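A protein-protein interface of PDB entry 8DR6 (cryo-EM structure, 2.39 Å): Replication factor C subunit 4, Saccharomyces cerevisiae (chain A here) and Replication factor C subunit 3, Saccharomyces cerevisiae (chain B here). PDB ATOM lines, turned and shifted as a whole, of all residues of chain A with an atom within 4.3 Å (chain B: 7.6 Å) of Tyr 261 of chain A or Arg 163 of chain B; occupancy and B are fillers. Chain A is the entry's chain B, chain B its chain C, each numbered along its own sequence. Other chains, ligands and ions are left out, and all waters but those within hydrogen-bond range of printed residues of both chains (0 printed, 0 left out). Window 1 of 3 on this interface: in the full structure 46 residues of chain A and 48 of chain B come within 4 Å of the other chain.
NH1 of Arg 165 of chain B lies within salt-bridge range of OD2 of Asp 229 of chain A (2.5 Å). O of Lys 259 of chain A sits at hydrogen-bond distance from NE of Arg 165 of chain B (2.7 Å). The side-chain hydroxyl (OH) of Tyr 261 of chain A is in hydrogen-bond range of the guanidinium group (NH2) of Arg 163 of chain B (3.4 Å). The backbone NH (N) of Ser 262 of chain A sits at hydrogen-bond distance from the side-chain hydroxyl (OH) of Tyr 52 of chain B.
The side-chain carboxylate of Asp 229 of chain A is in hydrogen-bond range of the side-chain hydroxyl of Ser 230 of chain A (3.3 Å). The backbone carbonyl oxygen of Leu 256 of chain A lies within hydrogen-bond range of the backbone NH of Tyr 261 of chain A, at 3.2 Å. The backbone carbonyl oxygen of Phe 164 of chain B lies within hydrogen-bond range of the backbone NH of Tyr 52 of chain B (2.9 Å). The backbone NH (N) of Phe 166 of chain B sits at hydrogen-bond distance from the backbone carbonyl oxygen (O) of Tyr 52 of chain B (2.9 Å).
Among the printed residues, merely in contact across the chains: Ser 262 of chain A with Tyr 149 of chain B (3.6 Å), Asp 229 of chain A with Arg 163 of chain B (3.7 Å), Tyr 261 of chain A with Tyr 52 of chain B (3.7 Å), Gly 260 of chain A with Pro 168 of chain B (3.7 Å), Lys 259 of chain A with Pro 168 of chain B (3.8 Å), Gly 260 of chain A with Pro 54 of chain B (3.8 Å), Ile 227 of chain A with Arg 163 of chain B (3.9 Å) and Tyr 261 of chain A with Arg 165 of chain B (3.9 Å).
Printed residues of chain B within 4 Å of Tyr 261 of chain A: Tyr 52, Arg 163 and Arg 165. Of chain A, only Ile 227 (3.9 Å), Asp 229 (3.7 Å) and Tyr 261 (3.4 Å) come within 4 Å of Arg 163 of chain B. Gly 260 of chain A touches just these residues of chain B: Pro 54 (3.8 Å) and Pro 168 (3.7 Å). Printed residues of chain B within 4 Å of Asp 229 of chain A: Arg 163 and Arg 165. Printed residues of chain A within 4 Å of Tyr 52 of chain B: Tyr 261 and Ser 262. Of the printed residues of chain A, Arg 165 of chain B touches Asp 229, Lys 259 and Tyr 261. Of the printed residues of chain A, Pro 54 of chain B touches Gly 260 (3.8 Å). Leu 158 of chain B touches none of the printed residues of chain A. The nearest residue of chain B that does not touch Tyr 261 of chain A is Pro 54 of chain B (5.8 Å). The nearest printed residue of chain A that does not touch Pro 54 of chain B is Lys 259 of chain A (5.6 Å).
Of the 12 printed residues of chain A, 6 touch a printed residue of chain B. Hydrophobic or aromatic side chains of chain A within 4 Å of the printed part of chain B: Tyr 261. Along chain A the printed residues that touch a printed residue of chain B span positions 227 to 262. Of the 22 printed residues of chain B, 6 touch a printed residue of chain A. Hydrophobic or aromatic side chains of chain B within 4 Å of the printed part of chain A: Tyr 52, Pro 54, Tyr 149 and Pro 168. Among the printed residues, 12 pairs touch across the chains.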
ATOM      1  N   ILE A 227       8.702 -13.577 -26.466  1.00  0.00           N
ATOM      2  CA  ILE A 227       7.924 -12.468 -27.013  1.00  0.00           C
ATOM      3  C   ILE A 227       7.213 -11.701 -25.901  1.00  0.00           C
ATOM      4  O   ILE A 227       7.279 -10.472 -25.842  1.00  0.00           O
ATOM      5  CB  ILE A 227       6.923 -12.966 -28.078  1.00  0.00           C
ATOM      6  CG1 ILE A 227       7.668 -13.397 -29.344  1.00  0.00           C
ATOM      7  CG2 ILE A 227       5.892 -11.890 -28.393  1.00  0.00           C
ATOM      8  CD1 ILE A 227       8.028 -12.252 -30.269  1.00  0.00           C
ATOM      9  N   ASP A 229       7.161 -10.862 -22.077  1.00  0.00           N
ATOM     10  CA  ASP A 229       7.997 -10.889 -20.888  1.00  0.00           C
ATOM     11  C   ASP A 229       7.159 -11.213 -19.658  1.00  0.00           C
ATOM     12  O   ASP A 229       5.943 -11.010 -19.639  1.00  0.00           O
ATOM     13  CB  ASP A 229       8.708  -9.548 -20.698  1.00  0.00           C
ATOM     14  CG  ASP A 229      10.001  -9.679 -19.916  1.00  0.00           C
ATOM     15  OD1 ASP A 229      10.237 -10.754 -19.325  1.00  0.00           O
ATOM     16  OD2 ASP A 229      10.785  -8.706 -19.895  1.00  0.00           O
ATOM     17  N   SER A 230       7.827 -11.724 -18.627  1.00  0.00           N
ATOM     18  CA  SER A 230       7.156 -12.076 -17.383  1.00  0.00           C
ATOM     19  C   SER A 230       6.523 -10.829 -16.775  1.00  0.00           C
ATOM     20  O   SER A 230       7.195  -9.798 -16.648  1.00  0.00           O
ATOM     21  CB  SER A 230       8.142 -12.707 -16.398  1.00  0.00           C
ATOM     22  OG  SER A 230       9.350 -11.970 -16.345  1.00  0.00           O
ATOM     23  N   HIS A 232       5.801  -7.944 -14.583  1.00  0.00           N
ATOM     24  CA  HIS A 232       6.582  -7.371 -13.494  1.00  0.00           C
ATOM     25  C   HIS A 232       5.772  -7.228 -12.207  1.00  0.00           C
ATOM     26  O   HIS A 232       6.363  -7.263 -11.119  1.00  0.00           O
ATOM     27  CB  HIS A 232       7.175  -6.019 -13.914  1.00  0.00           C
ATOM     28  CG  HIS A 232       6.171  -4.915 -14.024  1.00  0.00           C
ATOM     29  ND1 HIS A 232       5.516  -4.621 -15.200  1.00  0.00           N
ATOM     30  CD2 HIS A 232       5.719  -4.027 -13.109  1.00  0.00           C
ATOM     31  CE1 HIS A 232       4.698  -3.602 -15.003  1.00  0.00           C
ATOM     32  NE2 HIS A 232       4.802  -3.223 -13.742  1.00  0.00           N
ATOM     33  N   ASP A 255      16.033  -9.253 -11.039  1.00  0.00           N
ATOM     34  CA  ASP A 255      14.849  -9.360 -11.876  1.00  0.00           C
ATOM     35  C   ASP A 255      14.266  -8.019 -12.297  1.00  0.00           C
ATOM     36  O   ASP A 255      13.561  -7.965 -13.311  1.00  0.00           O
ATOM     37  CB  ASP A 255      13.762 -10.168 -11.150  1.00  0.00           C
ATOM     38  CG  ASP A 255      14.225 -11.561 -10.775  1.00  0.00           C
ATOM     39  OD1 ASP A 255      15.060 -12.130 -11.509  1.00  0.00           O
ATOM     40  OD2 ASP A 255      13.755 -12.088  -9.744  1.00  0.00           O
ATOM     41  N   LEU A 256      14.530  -6.942 -11.556  1.00  0.00           N
ATOM     42  CA  LEU A 256      13.916  -5.655 -11.859  1.00  0.00           C
ATOM     43  C   LEU A 256      14.950  -4.600 -12.234  1.00  0.00           C
ATOM     44  O   LEU A 256      14.847  -3.974 -13.294  1.00  0.00           O
ATOM     45  CB  LEU A 256      13.089  -5.174 -10.666  1.00  0.00           C
ATOM     46  CG  LEU A 256      11.859  -6.023 -10.333  1.00  0.00           C
ATOM     47  CD1 LEU A 256      11.303  -5.649  -8.969  1.00  0.00           C
ATOM     48  CD2 LEU A 256      10.793  -5.875 -11.408  1.00  0.00           C
ATOM     49  N   LYS A 259      17.229  -5.501 -15.266  1.00  0.00           N
ATOM     50  CA  LYS A 259      16.462  -5.695 -16.489  1.00  0.00           C
ATOM     51  C   LYS A 259      16.046  -4.384 -17.143  1.00  0.00           C
ATOM     52  O   LYS A 259      15.489  -4.409 -18.246  1.00  0.00           O
ATOM     53  CB  LYS A 259      15.212  -6.535 -16.201  1.00  0.00           C
ATOM     54  CG  LYS A 259      15.508  -7.896 -15.588  1.00  0.00           C
ATOM     55  CD  LYS A 259      16.413  -8.731 -16.486  1.00  0.00           C
ATOM     56  CE  LYS A 259      16.071 -10.214 -16.431  1.00  0.00           C
ATOM     57  NZ  LYS A 259      14.656 -10.501 -16.802  1.00  0.00           N
ATOM     58  N   GLY A 260      16.297  -3.250 -16.494  1.00  0.00           N
ATOM     59  CA  GLY A 260      15.993  -1.951 -17.056  1.00  0.00           C
ATOM     60  C   GLY A 260      14.735  -1.287 -16.536  1.00  0.00           C
ATOM     61  O   GLY A 260      14.393  -0.198 -17.012  1.00  0.00           O
ATOM     62  N   TYR A 261      14.034  -1.897 -15.584  1.00  0.00           N
ATOM     63  CA  TYR A 261      12.823  -1.292 -15.045  1.00  0.00           C
ATOM     64  C   TYR A 261      13.169  -0.047 -14.237  1.00  0.00           C
ATOM     65  O   TYR A 261      14.111  -0.052 -13.439  1.00  0.00           O
ATOM     66  CB  TYR A 261      12.071  -2.299 -14.177  1.00  0.00           C
ATOM     67  CG  TYR A 261      11.353  -3.367 -14.971  1.00  0.00           C
ATOM     68  CD1 TYR A 261      10.123  -3.113 -15.562  1.00  0.00           C
ATOM     69  CD2 TYR A 261      11.907  -4.630 -15.133  1.00  0.00           C
ATOM     70  CE1 TYR A 261       9.464  -4.085 -16.289  1.00  0.00           C
ATOM     71  CE2 TYR A 261      11.255  -5.609 -15.859  1.00  0.00           C
ATOM     72  CZ  TYR A 261      10.034  -5.331 -16.434  1.00  0.00           C
ATOM     73  OH  TYR A 261       9.381  -6.302 -17.158  1.00  0.00           O
ATOM     74  N   SER A 262      12.404   1.021 -14.448  1.00  0.00           N
ATOM     75  CA  SER A 262      12.660   2.278 -13.760  1.00  0.00           C
ATOM     76  C   SER A 262      12.209   2.202 -12.305  1.00  0.00           C
ATOM     77  O   SER A 262      11.329   1.418 -11.940  1.00  0.00           O
ATOM     78  CB  SER A 262      11.946   3.427 -14.469  1.00  0.00           C
ATOM     79  OG  SER A 262      10.541   3.323 -14.323  1.00  0.00           O
ATOM     80  N   SER A 263      12.828   3.038 -11.468  1.00  0.00           N
ATOM     81  CA  SER A 263      12.489   3.054 -10.048  1.00  0.00           C
ATOM     82  C   SER A 263      11.055   3.517  -9.827  1.00  0.00           C
ATOM     83  O   SER A 263      10.354   2.995  -8.951  1.00  0.00           O
ATOM     84  CB  SER A 263      13.465   3.950  -9.287  1.00  0.00           C
ATOM     85  OG  SER A 263      13.613   5.205  -9.930  1.00  0.00           O
ATOM     86  N   ILE A 266       8.778   0.697 -10.479  1.00  0.00           N
ATOM     87  CA  ILE A 266       8.876  -0.301  -9.418  1.00  0.00           C
ATOM     88  C   ILE A 266       8.082   0.138  -8.196  1.00  0.00           C
ATOM     89  O   ILE A 266       7.333  -0.652  -7.612  1.00  0.00           O
ATOM     90  CB  ILE A 266      10.353  -0.564  -9.068  1.00  0.00           C
ATOM     91  CG1 ILE A 266      11.071  -1.223 -10.249  1.00  0.00           C
ATOM     92  CG2 ILE A 266      10.458  -1.442  -7.829  1.00  0.00           C
ATOM     93  CD1 ILE A 266      12.574  -1.055 -10.220  1.00  0.00           C
ATOM     94  N   VAL B  33      15.891  -8.149 -29.823  1.00  0.00           N
ATOM     95  CA  VAL B  33      14.928  -7.205 -30.378  1.00  0.00           C
ATOM     96  C   VAL B  33      15.239  -6.923 -31.841  1.00  0.00           C
ATOM     97  O   VAL B  33      14.335  -6.884 -32.684  1.00  0.00           O
ATOM     98  CB  VAL B  33      14.914  -5.911 -29.545  1.00  0.00           C
ATOM     99  CG1 VAL B  33      13.963  -4.894 -30.156  1.00  0.00           C
ATOM    100  CG2 VAL B  33      14.531  -6.208 -28.100  1.00  0.00           C
ATOM    101  N   PRO B  47       3.977  -5.565 -36.496  1.00  0.00           N
ATOM    102  CA  PRO B  47       2.809  -5.149 -35.707  1.00  0.00           C
ATOM    103  C   PRO B  47       2.991  -3.772 -35.089  1.00  0.00           C
ATOM    104  O   PRO B  47       4.019  -3.122 -35.302  1.00  0.00           O
ATOM    105  CB  PRO B  47       2.723  -6.239 -34.636  1.00  0.00           C
ATOM    106  CG  PRO B  47       4.158  -6.573 -34.375  1.00  0.00           C
ATOM    107  CD  PRO B  47       4.883  -6.416 -35.702  1.00  0.00           C
ATOM    108  N   HIS B  48       2.002  -3.318 -34.324  1.00  0.00           N
ATOM    109  CA  HIS B  48       2.172  -2.105 -33.537  1.00  0.00           C
ATOM    110  C   HIS B  48       3.213  -2.359 -32.454  1.00  0.00           C
ATOM    111  O   HIS B  48       3.128  -3.348 -31.719  1.00  0.00           O
ATOM    112  CB  HIS B  48       0.842  -1.682 -32.916  1.00  0.00           C
ATOM    113  CG  HIS B  48      -0.230  -1.401 -33.923  1.00  0.00           C
ATOM    114  ND1 HIS B  48      -0.175  -0.334 -34.792  1.00  0.00           N
ATOM    115  CD2 HIS B  48      -1.385  -2.053 -34.200  1.00  0.00           C
ATOM    116  CE1 HIS B  48      -1.249  -0.338 -35.561  1.00  0.00           C
ATOM    117  NE2 HIS B  48      -2.000  -1.371 -35.221  1.00  0.00           N
ATOM    118  N   LEU B  49       4.195  -1.467 -32.353  1.00  0.00           N
ATOM    119  CA  LEU B  49       5.386  -1.712 -31.553  1.00  0.00           C
ATOM    120  C   LEU B  49       5.462  -0.751 -30.376  1.00  0.00           C
ATOM    121  O   LEU B  49       5.106   0.426 -30.491  1.00  0.00           O
ATOM    122  CB  LEU B  49       6.654  -1.576 -32.403  1.00  0.00           C
ATOM    123  CG  LEU B  49       6.908  -2.688 -33.425  1.00  0.00           C
ATOM    124  CD1 LEU B  49       8.117  -2.351 -34.282  1.00  0.00           C
ATOM    125  CD2 LEU B  49       7.096  -4.031 -32.737  1.00  0.00           C
ATOM    126  N   LEU B  50       5.932  -1.267 -29.243  1.00  0.00           N
ATOM    127  CA  LEU B  50       6.274  -0.466 -28.078  1.00  0.00           C
ATOM    128  C   LEU B  50       7.701  -0.817 -27.688  1.00  0.00           C
ATOM    129  O   LEU B  50       8.032  -1.996 -27.541  1.00  0.00           O
ATOM    130  CB  LEU B  50       5.307  -0.727 -26.920  1.00  0.00           C
ATOM    131  CG  LEU B  50       5.787  -0.375 -25.508  1.00  0.00           C
ATOM    132  CD1 LEU B  50       6.086   1.111 -25.386  1.00  0.00           C
ATOM    133  CD2 LEU B  50       4.751  -0.797 -24.480  1.00  0.00           C
ATOM    134  N   PHE B  51       8.547   0.198 -27.558  1.00  0.00           N
ATOM    135  CA  PHE B  51       9.926   0.032 -27.118  1.00  0.00           C
ATOM    136  C   PHE B  51      10.073   0.678 -25.747  1.00  0.00           C
ATOM    137  O   PHE B  51      10.110   1.909 -25.638  1.00  0.00           O
ATOM    138  CB  PHE B  51      10.902   0.663 -28.113  1.00  0.00           C
ATOM    139  CG  PHE B  51      11.006  -0.069 -29.429  1.00  0.00           C
ATOM    140  CD1 PHE B  51      10.342  -1.269 -29.641  1.00  0.00           C
ATOM    141  CD2 PHE B  51      11.774   0.453 -30.457  1.00  0.00           C
ATOM    142  CE1 PHE B  51      10.446  -1.930 -30.850  1.00  0.00           C
ATOM    143  CE2 PHE B  51      11.880  -0.206 -31.668  1.00  0.00           C
ATOM    144  CZ  PHE B  51      11.215  -1.397 -31.864  1.00  0.00           C
ATOM    145  N   TYR B  52      10.155  -0.147 -24.706  1.00  0.00           N
ATOM    146  CA  TYR B  52      10.277   0.335 -23.339  1.00  0.00           C
ATOM    147  C   TYR B  52      11.691   0.078 -22.842  1.00  0.00           C
ATOM    148  O   TYR B  52      12.193  -1.046 -22.936  1.00  0.00           O
ATOM    149  CB  TYR B  52       9.259  -0.351 -22.420  1.00  0.00           C
ATOM    150  CG  TYR B  52       9.500  -0.113 -20.947  1.00  0.00           C
ATOM    151  CD1 TYR B  52       9.074   1.058 -20.334  1.00  0.00           C
ATOM    152  CD2 TYR B  52      10.149  -1.061 -20.167  1.00  0.00           C
ATOM    153  CE1 TYR B  52       9.290   1.279 -18.989  1.00  0.00           C
ATOM    154  CE2 TYR B  52      10.370  -0.849 -18.820  1.00  0.00           C
ATOM    155  CZ  TYR B  52       9.938   0.324 -18.236  1.00  0.00           C
ATOM    156  OH  TYR B  52      10.156   0.541 -16.895  1.00  0.00           O
ATOM    157  N   GLY B  53      12.335   1.117 -22.319  1.00  0.00           N
ATOM    158  CA  GLY B  53      13.690   0.964 -21.838  1.00  0.00           C
ATOM    159  C   GLY B  53      14.243   2.172 -21.113  1.00  0.00           C
ATOM    160  O   GLY B  53      13.667   3.263 -21.137  1.00  0.00           O
ATOM    161  N   PRO B  54      15.385   1.995 -20.455  1.00  0.00           N
ATOM    162  CA  PRO B  54      16.009   3.104 -19.728  1.00  0.00           C
ATOM    163  C   PRO B  54      16.753   4.030 -20.672  1.00  0.00           C
ATOM    164  O   PRO B  54      16.889   3.734 -21.869  1.00  0.00           O
ATOM    165  CB  PRO B  54      16.971   2.395 -18.763  1.00  0.00           C
ATOM    166  CG  PRO B  54      17.315   1.120 -19.444  1.00  0.00           C
ATOM    167  CD  PRO B  54      16.135   0.735 -20.301  1.00  0.00           C
ATOM    168  N   ASN B 148      10.201   5.390 -21.512  1.00  0.00           N
ATOM    169  CA  ASN B 148      11.089   5.101 -20.396  1.00  0.00           C
ATOM    170  C   ASN B 148      10.335   4.713 -19.132  1.00  0.00           C
ATOM    171  O   ASN B 148      10.897   4.009 -18.286  1.00  0.00           O
ATOM    172  CB  ASN B 148      11.972   6.318 -20.088  1.00  0.00           C
ATOM    173  CG  ASN B 148      13.003   6.583 -21.168  1.00  0.00           C
ATOM    174  OD1 ASN B 148      13.053   7.672 -21.739  1.00  0.00           O
ATOM    175  ND2 ASN B 148      13.843   5.592 -21.441  1.00  0.00           N
ATOM    176  N   TYR B 149       9.086   5.155 -18.989  1.00  0.00           N
ATOM    177  CA  TYR B 149       8.262   4.861 -17.819  1.00  0.00           C
ATOM    178  C   TYR B 149       6.931   4.306 -18.308  1.00  0.00           C
ATOM    179  O   TYR B 149       6.163   5.016 -18.965  1.00  0.00           O
ATOM    180  CB  TYR B 149       8.051   6.112 -16.967  1.00  0.00           C
ATOM    181  CG  TYR B 149       9.296   6.954 -16.800  1.00  0.00           C
ATOM    182  CD1 TYR B 149      10.330   6.542 -15.969  1.00  0.00           C
ATOM    183  CD2 TYR B 149       9.438   8.159 -17.473  1.00  0.00           C
ATOM    184  CE1 TYR B 149      11.470   7.307 -15.814  1.00  0.00           C
ATOM    185  CE2 TYR B 149      10.573   8.932 -17.325  1.00  0.00           C
ATOM    186  CZ  TYR B 149      11.586   8.502 -16.494  1.00  0.00           C
ATOM    187  OH  TYR B 149      12.719   9.267 -16.344  1.00  0.00           O
ATOM    188  N   ALA B 150       6.656   3.041 -17.985  1.00  0.00           N
ATOM    189  CA  ALA B 150       5.428   2.398 -18.436  1.00  0.00           C
ATOM    190  C   ALA B 150       4.204   2.829 -17.637  1.00  0.00           C
ATOM    191  O   ALA B 150       3.080   2.681 -18.130  1.00  0.00           O
ATOM    192  CB  ALA B 150       5.575   0.877 -18.360  1.00  0.00           C
ATOM    193  N   LEU B 158      -1.501   0.193 -24.093  1.00  0.00           N
ATOM    194  CA  LEU B 158      -0.586  -0.935 -23.959  1.00  0.00           C
ATOM    195  C   LEU B 158      -1.176  -2.209 -24.549  1.00  0.00           C
ATOM    196  O   LEU B 158      -0.450  -3.001 -25.161  1.00  0.00           O
ATOM    197  CB  LEU B 158      -0.234  -1.151 -22.488  1.00  0.00           C
ATOM    198  CG  LEU B 158       0.682  -0.098 -21.861  1.00  0.00           C
ATOM    199  CD1 LEU B 158       0.585  -0.139 -20.344  1.00  0.00           C
ATOM    200  CD2 LEU B 158       2.119  -0.300 -22.313  1.00  0.00           C
ATOM    201  N   ARG B 160      -2.887  -2.636 -27.107  1.00  0.00           N
ATOM    202  CA  ARG B 160      -2.889  -2.636 -28.564  1.00  0.00           C
ATOM    203  C   ARG B 160      -1.500  -2.761 -29.177  1.00  0.00           C
ATOM    204  O   ARG B 160      -1.391  -2.810 -30.407  1.00  0.00           O
ATOM    205  CB  ARG B 160      -3.549  -1.355 -29.090  1.00  0.00           C
ATOM    206  CG  ARG B 160      -5.054  -1.297 -28.896  1.00  0.00           C
ATOM    207  CD  ARG B 160      -5.570   0.127 -29.026  1.00  0.00           C
ATOM    208  NE  ARG B 160      -7.026   0.187 -29.079  1.00  0.00           N
ATOM    209  CZ  ARG B 160      -7.823   0.016 -28.034  1.00  0.00           C
ATOM    210  NH1 ARG B 160      -7.340  -0.234 -26.827  1.00  0.00           N
ATOM    211  NH2 ARG B 160      -9.140   0.097 -28.202  1.00  0.00           N
ATOM    212  N   CYS B 161      -0.446  -2.817 -28.367  1.00  0.00           N
ATOM    213  CA  CYS B 161       0.922  -2.818 -28.863  1.00  0.00           C
ATOM    214  C   CYS B 161       1.684  -4.030 -28.341  1.00  0.00           C
ATOM    215  O   CYS B 161       1.432  -4.518 -27.236  1.00  0.00           O
ATOM    216  CB  CYS B 161       1.654  -1.537 -28.449  1.00  0.00           C
ATOM    217  SG  CYS B 161       1.061  -0.043 -29.276  1.00  0.00           S
ATOM    218  N   THR B 162       2.622  -4.509 -29.156  1.00  0.00           N
ATOM    219  CA  THR B 162       3.529  -5.577 -28.760  1.00  0.00           C
ATOM    220  C   THR B 162       4.777  -4.955 -28.145  1.00  0.00           C
ATOM    221  O   THR B 162       5.386  -4.059 -28.738  1.00  0.00           O
ATOM    222  CB  THR B 162       3.901  -6.450 -29.960  1.00  0.00           C
ATOM    223  OG1 THR B 162       2.762  -7.219 -30.365  1.00  0.00           O
ATOM    224  CG2 THR B 162       5.041  -7.394 -29.609  1.00  0.00           C
ATOM    225  N   ARG B 163       5.154  -5.435 -26.964  1.00  0.00           N
ATOM    226  CA  ARG B 163       6.163  -4.787 -26.137  1.00  0.00           C
ATOM    227  C   ARG B 163       7.536  -5.414 -26.346  1.00  0.00           C
ATOM    228  O   ARG B 163       7.665  -6.637 -26.460  1.00  0.00           O
ATOM    229  CB  ARG B 163       5.775  -4.874 -24.659  1.00  0.00           C
ATOM    230  CG  ARG B 163       6.786  -4.258 -23.707  1.00  0.00           C
ATOM    231  CD  ARG B 163       6.189  -4.072 -22.322  1.00  0.00           C
ATOM    232  NE  ARG B 163       7.204  -3.780 -21.316  1.00  0.00           N
ATOM    233  CZ  ARG B 163       7.971  -4.693 -20.736  1.00  0.00           C
ATOM    234  NH1 ARG B 163       7.874  -5.977 -21.044  1.00  0.00           N
ATOM    235  NH2 ARG B 163       8.858  -4.310 -19.823  1.00  0.00           N
ATOM    236  N   PHE B 164       8.559  -4.561 -26.396  1.00  0.00           N
ATOM    237  CA  PHE B 164       9.953  -4.978 -26.469  1.00  0.00           C
ATOM    238  C   PHE B 164      10.731  -4.197 -25.421  1.00  0.00           C
ATOM    239  O   PHE B 164      10.678  -2.962 -25.396  1.00  0.00           O
ATOM    240  CB  PHE B 164      10.541  -4.730 -27.862  1.00  0.00           C
ATOM    241  CG  PHE B 164      10.065  -5.698 -28.906  1.00  0.00           C
ATOM    242  CD1 PHE B 164       8.839  -5.524 -29.525  1.00  0.00           C
ATOM    243  CD2 PHE B 164      10.848  -6.780 -29.274  1.00  0.00           C
ATOM    244  CE1 PHE B 164       8.402  -6.412 -30.488  1.00  0.00           C
ATOM    245  CE2 PHE B 164      10.415  -7.671 -30.236  1.00  0.00           C
ATOM    246  CZ  PHE B 164       9.190  -7.487 -30.844  1.00  0.00           C
ATOM    247  N   ARG B 165      11.465  -4.915 -24.575  1.00  0.00           N
ATOM    248  CA  ARG B 165      12.219  -4.308 -23.488  1.00  0.00           C
ATOM    249  C   ARG B 165      13.681  -4.166 -23.896  1.00  0.00           C
ATOM    250  O   ARG B 165      14.320  -5.149 -24.286  1.00  0.00           O
ATOM    251  CB  ARG B 165      12.102  -5.147 -22.216  1.00  0.00           C
ATOM    252  CG  ARG B 165      12.054  -4.325 -20.938  1.00  0.00           C
ATOM    253  CD  ARG B 165      12.222  -5.194 -19.702  1.00  0.00           C
ATOM    254  NE  ARG B 165      13.559  -5.772 -19.611  1.00  0.00           N
ATOM    255  CZ  ARG B 165      13.885  -6.998 -20.004  1.00  0.00           C
ATOM    256  NH1 ARG B 165      12.993  -7.819 -20.533  1.00  0.00           N
ATOM    257  NH2 ARG B 165      15.142  -7.409 -19.866  1.00  0.00           N
ATOM    258  N   PHE B 166      14.201  -2.947 -23.807  1.00  0.00           N
ATOM    259  CA  PHE B 166      15.610  -2.683 -24.061  1.00  0.00           C
ATOM    260  C   PHE B 166      16.386  -2.780 -22.753  1.00  0.00           C
ATOM    261  O   PHE B 166      16.196  -1.960 -21.848  1.00  0.00           O
ATOM    262  CB  PHE B 166      15.801  -1.302 -24.691  1.00  0.00           C
ATOM    263  CG  PHE B 166      15.541  -1.271 -26.170  1.00  0.00           C
ATOM    264  CD1 PHE B 166      14.273  -1.514 -26.672  1.00  0.00           C
ATOM    265  CD2 PHE B 166      16.567  -0.997 -27.060  1.00  0.00           C
ATOM    266  CE1 PHE B 166      14.034  -1.485 -28.032  1.00  0.00           C
ATOM    267  CE2 PHE B 166      16.333  -0.966 -28.421  1.00  0.00           C
ATOM    268  CZ  PHE B 166      15.065  -1.211 -28.908  1.00  0.00           C
ATOM    269  N   GLN B 167      17.250  -3.780 -22.658  1.00  0.00           N
ATOM    270  CA  GLN B 167      18.022  -4.033 -21.454  1.00  0.00           C
ATOM    271  C   GLN B 167      19.193  -3.067 -21.350  1.00  0.00           C
ATOM    272  O   GLN B 167      19.604  -2.461 -22.345  1.00  0.00           O
ATOM    273  CB  GLN B 167      18.538  -5.470 -21.456  1.00  0.00           C
ATOM    274  CG  GLN B 167      19.595  -5.744 -22.520  1.00  0.00           C
ATOM    275  CD  GLN B 167      20.052  -7.187 -22.535  1.00  0.00           C
ATOM    276  OE1 GLN B 167      19.695  -7.974 -21.658  1.00  0.00           O
ATOM    277  NE2 GLN B 167      20.852  -7.543 -23.534  1.00  0.00           N
ATOM    278  N   PRO B 168      19.753  -2.894 -20.153  1.00  0.00           N
ATOM    279  CA  PRO B 168      21.016  -2.159 -20.043  1.00  0.00           C
ATOM    280  C   PRO B 168      22.095  -2.819 -20.888  1.00  0.00           C
ATOM    281  O   PRO B 168      22.169  -4.046 -20.986  1.00  0.00           O
ATOM    282  CB  PRO B 168      21.339  -2.230 -18.547  1.00  0.00           C
ATOM    283  CG  PRO B 168      20.016  -2.417 -17.887  1.00  0.00           C
ATOM    284  CD  PRO B 168      19.211  -3.259 -18.833  1.00  0.00           C
